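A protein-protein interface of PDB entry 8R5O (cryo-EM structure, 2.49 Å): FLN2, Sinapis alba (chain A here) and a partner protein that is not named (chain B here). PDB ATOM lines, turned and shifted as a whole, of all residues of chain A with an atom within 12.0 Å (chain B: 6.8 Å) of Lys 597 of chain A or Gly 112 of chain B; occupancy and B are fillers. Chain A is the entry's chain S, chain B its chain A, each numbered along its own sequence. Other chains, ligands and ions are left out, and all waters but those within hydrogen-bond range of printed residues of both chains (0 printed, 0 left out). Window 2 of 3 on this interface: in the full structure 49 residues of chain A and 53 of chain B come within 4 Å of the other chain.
Glu 594 of chain A touches none of the printed residues of chain B. Of the printed residues of chain B, Tyr 595 of chain A touches Cys 109 (3.3 Å) and Asn 144 (3.7 Å). Printed residues of chain B within 4 Å of Arg 596 of chain A: Cys 109, Val 110 and Gln 111. Lys 597 of chain A touches one residue of chain B. Printed residues of chain B within 4 Å of Leu 598 of chain A: Val 110, Gln 111, Gly 112 and Leu 139. Of the printed residues of chain A, Cys 109 of chain B touches Tyr 595 and Arg 596. Of the printed residues of chain A, Val 110 of chain B touches Arg 596 and Leu 598. Gln 111 of chain B touches just these residues of chain A: Arg 596 (3.3 Å) and Leu 598 (3.3 Å). Gly 112 of chain B touches just these residues of chain A: Lys 597 (3.5 Å) and Leu 598 (3.97 Å). No residue of chain A comes within 4 Å of Pro 113 of chain B. No residue of chain A comes within 4 Å of Gly 114 of chain B. Of chain A, only Leu 598 comes within 4 Å of Leu 139 of chain B. No residue of chain A comes within 4 Å of Ile 143 of chain B. Asn 144 of chain B touches just one residue of chain A: Tyr 595. The nearest residue of chain B that does not touch Lys 597 of chain A is Gln 111 of chain B (4.1 Å). The nearest printed residue of chain B that does not touch Tyr 595 of chain A is Val 110 of chain B (4.03 Å).
O of Arg 596 of chain A sits at hydrogen-bond distance from N of Gln 111 of chain B (3.3 Å). O of Gln 111 of chain B lies close to N of Leu 598 of chain A (3.4 Å). The side-chain amino group of Lys 597 of chain A is in hydrogen-bond range of the backbone carbonyl oxygen of Gly 112 of chain B, 3.5 Å away. The backbone carbonyl oxygen of Cys 109 of chain B sits at hydrogen-bond distance from the backbone NH of Arg 596 of chain A (3.3 Å).
Printed residues of chain B that touch a printed residue of chain A: Cys 109, Val 110, Gln 111, Gly 112, Leu 139 and Asn 144. Hydrophobic or aromatic side chains of chain B within 4 Å of the printed part of chain A: Val 110 and Leu 139. Hydrophobic or aromatic side chains of chain A that line the printed part of chain B: Tyr 595 and Leu 598.
NH1 of Arg 593 of chain A lies within hydrogen-bond range of OH of Tyr 595 of chain A, 2.6 Å away. The backbone carbonyl oxygen (O) of Ile 143 of chain B lies within hydrogen-bond range of the backbone NH (N) of Gly 112 of chain B (3.0 Å). NE2 of Gln 111 of chain B lies close to OD1 of Asn 144 of chain B (3.1 Å). O of Val 110 of chain B is in hydrogen-bond range of N of Leu 145 of chain B (3.1 Å). The backbone NH of Leu 139 of chain B is in hydrogen-bond range of the backbone carbonyl oxygen of Gly 114 of chain B (2.8 Å).
Tyr 595 of chain A touches Cys 109 of chain B (CD1 to SG, 3.3 Å). Asn 144 of chain B touches Tyr 595 of chain A. O of Arg 596 of chain A touches CA of Val 110 of chain B (3.5 Å). Val 110 of chain B touches Leu 598 of chain A (CG1 to CD2, 3.6 Å). Leu 598 of chain A touches Gly 112 of chain B (CD1 to CA, 3.97 Å). CD1 of Leu 598 of chain A touches CD1 of Leu 139 of chain B, at 3.7 Å.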
ATOM      1  N   ARG A 593      17.735 -17.468   5.433  1.00  0.00           N
ATOM      2  CA  ARG A 593      16.518 -18.263   5.329  1.00  0.00           C
ATOM      3  C   ARG A 593      16.386 -18.942   3.973  1.00  0.00           C
ATOM      4  O   ARG A 593      16.248 -20.169   3.918  1.00  0.00           O
ATOM      5  CB  ARG A 593      15.293 -17.386   5.613  1.00  0.00           C
ATOM      6  CG  ARG A 593      15.076 -17.083   7.084  1.00  0.00           C
ATOM      7  CD  ARG A 593      14.674 -18.334   7.847  1.00  0.00           C
ATOM      8  NE  ARG A 593      14.479 -18.073   9.268  1.00  0.00           N
ATOM      9  CZ  ARG A 593      13.351 -17.623   9.799  1.00  0.00           C
ATOM     10  NH1 ARG A 593      12.293 -17.355   9.051  1.00  0.00           N
ATOM     11  NH2 ARG A 593      13.283 -17.436  11.113  1.00  0.00           N
ATOM     12  N   GLU A 594      16.430 -18.183   2.879  1.00  0.00           N
ATOM     13  CA  GLU A 594      16.168 -18.696   1.536  1.00  0.00           C
ATOM     14  C   GLU A 594      14.819 -19.418   1.486  1.00  0.00           C
ATOM     15  O   GLU A 594      14.728 -20.630   1.282  1.00  0.00           O
ATOM     16  CB  GLU A 594      17.301 -19.612   1.057  1.00  0.00           C
ATOM     17  CG  GLU A 594      18.631 -18.910   0.831  1.00  0.00           C
ATOM     18  CD  GLU A 594      19.679 -19.303   1.854  1.00  0.00           C
ATOM     19  OE1 GLU A 594      19.366 -19.294   3.063  1.00  0.00           O
ATOM     20  OE2 GLU A 594      20.812 -19.629   1.449  1.00  0.00           O
ATOM     21  N   TYR A 595      13.765 -18.631   1.705  1.00  0.00           N
ATOM     22  CA  TYR A 595      12.404 -19.148   1.658  1.00  0.00           C
ATOM     23  C   TYR A 595      12.126 -19.768   0.297  1.00  0.00           C
ATOM     24  O   TYR A 595      12.085 -19.063  -0.717  1.00  0.00           O
ATOM     25  CB  TYR A 595      11.392 -18.041   1.959  1.00  0.00           C
ATOM     26  CG  TYR A 595      11.542 -17.425   3.330  1.00  0.00           C
ATOM     27  CD1 TYR A 595      10.978 -18.026   4.446  1.00  0.00           C
ATOM     28  CD2 TYR A 595      12.243 -16.240   3.509  1.00  0.00           C
ATOM     29  CE1 TYR A 595      11.111 -17.468   5.704  1.00  0.00           C
ATOM     30  CE2 TYR A 595      12.378 -15.673   4.760  1.00  0.00           C
ATOM     31  CZ  TYR A 595      11.813 -16.290   5.854  1.00  0.00           C
ATOM     32  OH  TYR A 595      11.947 -15.728   7.102  1.00  0.00           O
ATOM     33  N   ARG A 596      11.940 -21.085   0.269  1.00  0.00           N
ATOM     34  CA  ARG A 596      11.766 -21.805  -0.984  1.00  0.00           C
ATOM     35  C   ARG A 596      10.450 -21.406  -1.638  1.00  0.00           C
ATOM     36  O   ARG A 596       9.375 -21.599  -1.059  1.00  0.00           O
ATOM     37  CB  ARG A 596      11.814 -23.308  -0.727  1.00  0.00           C
ATOM     38  CG  ARG A 596      13.063 -23.754   0.015  1.00  0.00           C
ATOM     39  CD  ARG A 596      12.915 -25.157   0.582  1.00  0.00           C
ATOM     40  NE  ARG A 596      12.729 -26.158  -0.460  1.00  0.00           N
ATOM     41  CZ  ARG A 596      13.720 -26.771  -1.094  1.00  0.00           C
ATOM     42  NH1 ARG A 596      14.985 -26.492  -0.831  1.00  0.00           N
ATOM     43  NH2 ARG A 596      13.432 -27.685  -2.015  1.00  0.00           N
ATOM     44  N   LYS A 597      10.539 -20.844  -2.841  1.00  0.00           N
ATOM     45  CA  LYS A 597       9.351 -20.396  -3.552  1.00  0.00           C
ATOM     46  C   LYS A 597       8.479 -21.581  -3.940  1.00  0.00           C
ATOM     47  O   LYS A 597       8.973 -22.612  -4.406  1.00  0.00           O
ATOM     48  CB  LYS A 597       9.750 -19.607  -4.800  1.00  0.00           C
ATOM     49  CG  LYS A 597       8.602 -18.881  -5.478  1.00  0.00           C
ATOM     50  CD  LYS A 597       8.181 -17.653  -4.687  1.00  0.00           C
ATOM     51  CE  LYS A 597       7.271 -16.753  -5.506  1.00  0.00           C
ATOM     52  NZ  LYS A 597       6.999 -15.459  -4.819  1.00  0.00           N
ATOM     53  N   LEU A 598       7.173 -21.429  -3.750  1.00  0.00           N
ATOM     54  CA  LEU A 598       6.226 -22.490  -4.067  1.00  0.00           C
ATOM     55  C   LEU A 598       5.970 -22.562  -5.568  1.00  0.00           C
ATOM     56  O   LEU A 598       4.873 -22.904  -6.003  1.00  0.00           O
ATOM     57  CB  LEU A 598       4.911 -22.277  -3.318  1.00  0.00           C
ATOM     58  CG  LEU A 598       4.988 -22.263  -1.790  1.00  0.00           C
ATOM     59  CD1 LEU A 598       3.659 -21.836  -1.193  1.00  0.00           C
ATOM     60  CD2 LEU A 598       5.397 -23.630  -1.266  1.00  0.00           C
ATOM     61  N   CYS B 109       9.595 -24.122   5.267  1.00  0.00           N
ATOM     62  CA  CYS B 109      10.057 -22.753   5.035  1.00  0.00           C
ATOM     63  C   CYS B 109       9.695 -22.398   3.597  1.00  0.00           C
ATOM     64  O   CYS B 109      10.415 -22.760   2.663  1.00  0.00           O
ATOM     65  CB  CYS B 109      11.555 -22.622   5.287  1.00  0.00           C
ATOM     66  SG  CYS B 109      12.138 -20.923   5.478  1.00  0.00           S
ATOM     67  N   VAL B 110       8.573 -21.697   3.426  1.00  0.00           N
ATOM     68  CA  VAL B 110       7.991 -21.457   2.112  1.00  0.00           C
ATOM     69  C   VAL B 110       7.593 -19.993   1.985  1.00  0.00           C
ATOM     70  O   VAL B 110       7.438 -19.275   2.974  1.00  0.00           O
ATOM     71  CB  VAL B 110       6.761 -22.354   1.852  1.00  0.00           C
ATOM     72  CG1 VAL B 110       7.161 -23.820   1.819  1.00  0.00           C
ATOM     73  CG2 VAL B 110       5.699 -22.108   2.910  1.00  0.00           C
ATOM     74  N   GLN B 111       7.429 -19.560   0.737  1.00  0.00           N
ATOM     75  CA  GLN B 111       6.918 -18.234   0.418  1.00  0.00           C
ATOM     76  C   GLN B 111       5.773 -18.386  -0.570  1.00  0.00           C
ATOM     77  O   GLN B 111       5.902 -19.103  -1.567  1.00  0.00           O
ATOM     78  CB  GLN B 111       8.020 -17.338  -0.162  1.00  0.00           C
ATOM     79  CG  GLN B 111       7.635 -15.873  -0.277  1.00  0.00           C
ATOM     80  CD  GLN B 111       8.837 -14.968  -0.470  1.00  0.00           C
ATOM     81  OE1 GLN B 111       9.935 -15.434  -0.774  1.00  0.00           O
ATOM     82  NE2 GLN B 111       8.636 -13.668  -0.283  1.00  0.00           N
ATOM     83  N   GLY B 112       4.659 -17.716  -0.293  1.00  0.00           N
ATOM     84  CA  GLY B 112       3.463 -17.870  -1.089  1.00  0.00           C
ATOM     85  C   GLY B 112       3.430 -16.957  -2.296  1.00  0.00           C
ATOM     86  O   GLY B 112       4.408 -16.275  -2.616  1.00  0.00           O
ATOM     87  N   PRO B 113       2.293 -16.931  -3.002  1.00  0.00           N
ATOM     88  CA  PRO B 113       1.073 -17.722  -2.780  1.00  0.00           C
ATOM     89  C   PRO B 113       1.183 -19.126  -3.365  1.00  0.00           C
ATOM     90  O   PRO B 113       2.043 -19.383  -4.203  1.00  0.00           O
ATOM     91  CB  PRO B 113       0.002 -16.888  -3.491  1.00  0.00           C
ATOM     92  CG  PRO B 113       0.742 -16.290  -4.651  1.00  0.00           C
ATOM     93  CD  PRO B 113       2.125 -15.988  -4.123  1.00  0.00           C
ATOM     94  N   GLY B 114       0.334 -20.054  -2.949  1.00  0.00           N
ATOM     95  CA  GLY B 114       0.354 -21.385  -3.515  1.00  0.00           C
ATOM     96  C   GLY B 114      -0.270 -22.393  -2.570  1.00  0.00           C
ATOM     97  O   GLY B 114      -0.941 -22.040  -1.601  1.00  0.00           O
ATOM     98  N   LEU B 139      -1.973 -20.651   0.605  1.00  0.00           N
ATOM     99  CA  LEU B 139      -1.430 -19.304   0.724  1.00  0.00           C
ATOM    100  C   LEU B 139      -2.019 -18.430  -0.376  1.00  0.00           C
ATOM    101  O   LEU B 139      -1.870 -18.737  -1.564  1.00  0.00           O
ATOM    102  CB  LEU B 139       0.095 -19.320   0.640  1.00  0.00           C
ATOM    103  CG  LEU B 139       0.842 -19.754   1.899  1.00  0.00           C
ATOM    104  CD1 LEU B 139       2.324 -19.914   1.624  1.00  0.00           C
ATOM    105  CD2 LEU B 139       0.620 -18.746   3.004  1.00  0.00           C
ATOM    106  N   THR B 140      -2.687 -17.347   0.021  1.00  0.00           N
ATOM    107  CA  THR B 140      -3.310 -16.420  -0.915  1.00  0.00           C
ATOM    108  C   THR B 140      -2.559 -15.096  -1.002  1.00  0.00           C
ATOM    109  O   THR B 140      -3.112 -14.104  -1.487  1.00  0.00           O
ATOM    110  CB  THR B 140      -4.766 -16.169  -0.525  1.00  0.00           C
ATOM    111  OG1 THR B 140      -4.812 -15.442   0.708  1.00  0.00           O
ATOM    112  CG2 THR B 140      -5.503 -17.487  -0.352  1.00  0.00           C
ATOM    113  N   GLU B 141      -1.310 -15.059  -0.543  1.00  0.00           N
ATOM    114  CA  GLU B 141      -0.544 -13.823  -0.503  1.00  0.00           C
ATOM    115  C   GLU B 141       0.932 -14.174  -0.441  1.00  0.00           C
ATOM    116  O   GLU B 141       1.302 -15.155   0.213  1.00  0.00           O
ATOM    117  CB  GLU B 141      -0.950 -12.970   0.708  1.00  0.00           C
ATOM    118  CG  GLU B 141      -0.539 -11.513   0.634  1.00  0.00           C
ATOM    119  CD  GLU B 141      -1.470 -10.618   1.424  1.00  0.00           C
ATOM    120  OE1 GLU B 141      -2.556 -11.094   1.818  1.00  0.00           O
ATOM    121  OE2 GLU B 141      -1.120  -9.439   1.648  1.00  0.00           O
ATOM    122  N   PRO B 142       1.800 -13.405  -1.109  1.00  0.00           N
ATOM    123  CA  PRO B 142       3.241 -13.684  -1.034  1.00  0.00           C
ATOM    124  C   PRO B 142       3.824 -13.378   0.335  1.00  0.00           C
ATOM    125  O   PRO B 142       4.503 -12.361   0.514  1.00  0.00           O
ATOM    126  CB  PRO B 142       3.836 -12.764  -2.111  1.00  0.00           C
ATOM    127  CG  PRO B 142       2.695 -12.440  -3.018  1.00  0.00           C
ATOM    128  CD  PRO B 142       1.489 -12.396  -2.136  1.00  0.00           C
ATOM    129  N   ILE B 143       3.570 -14.247   1.306  1.00  0.00           N
ATOM    130  CA  ILE B 143       4.066 -14.071   2.660  1.00  0.00           C
ATOM    131  C   ILE B 143       5.115 -15.142   2.948  1.00  0.00           C
ATOM    132  O   ILE B 143       5.286 -16.099   2.194  1.00  0.00           O
ATOM    133  CB  ILE B 143       2.934 -14.113   3.704  1.00  0.00           C
ATOM    134  CG1 ILE B 143       2.325 -15.514   3.774  1.00  0.00           C
ATOM    135  CG2 ILE B 143       1.868 -13.081   3.374  1.00  0.00           C
ATOM    136  CD1 ILE B 143       1.346 -15.691   4.906  1.00  0.00           C
ATOM    137  N   ASN B 144       5.822 -14.968   4.060  1.00  0.00           N
ATOM    138  CA  ASN B 144       6.826 -15.919   4.513  1.00  0.00           C
ATOM    139  C   ASN B 144       6.270 -16.716   5.684  1.00  0.00           C
ATOM    140  O   ASN B 144       5.803 -16.136   6.670  1.00  0.00           O
ATOM    141  CB  ASN B 144       8.112 -15.203   4.927  1.00  0.00           C
ATOM    142  CG  ASN B 144       8.765 -14.468   3.777  1.00  0.00           C
ATOM    143  OD1 ASN B 144       8.614 -14.849   2.617  1.00  0.00           O
ATOM    144  ND2 ASN B 144       9.500 -13.409   4.092  1.00  0.00           N
ATOM    145  N   LEU B 145       6.319 -18.041   5.574  1.00  0.00           N
ATOM    146  CA  LEU B 145       5.804 -18.932   6.605  1.00  0.00           C
ATOM    147  C   LEU B 145       6.873 -19.951   6.957  1.00  0.00           C
ATOM    148  O   LEU B 145       7.270 -20.753   6.107  1.00  0.00           O
ATOM    149  CB  LEU B 145       4.523 -19.633   6.142  1.00  0.00           C
ATOM    150  CG  LEU B 145       3.844 -20.501   7.200  1.00  0.00           C
ATOM    151  CD1 LEU B 145       3.477 -19.662   8.413  1.00  0.00           C
ATOM    152  CD2 LEU B 145       2.618 -21.197   6.627  1.00  0.00           C
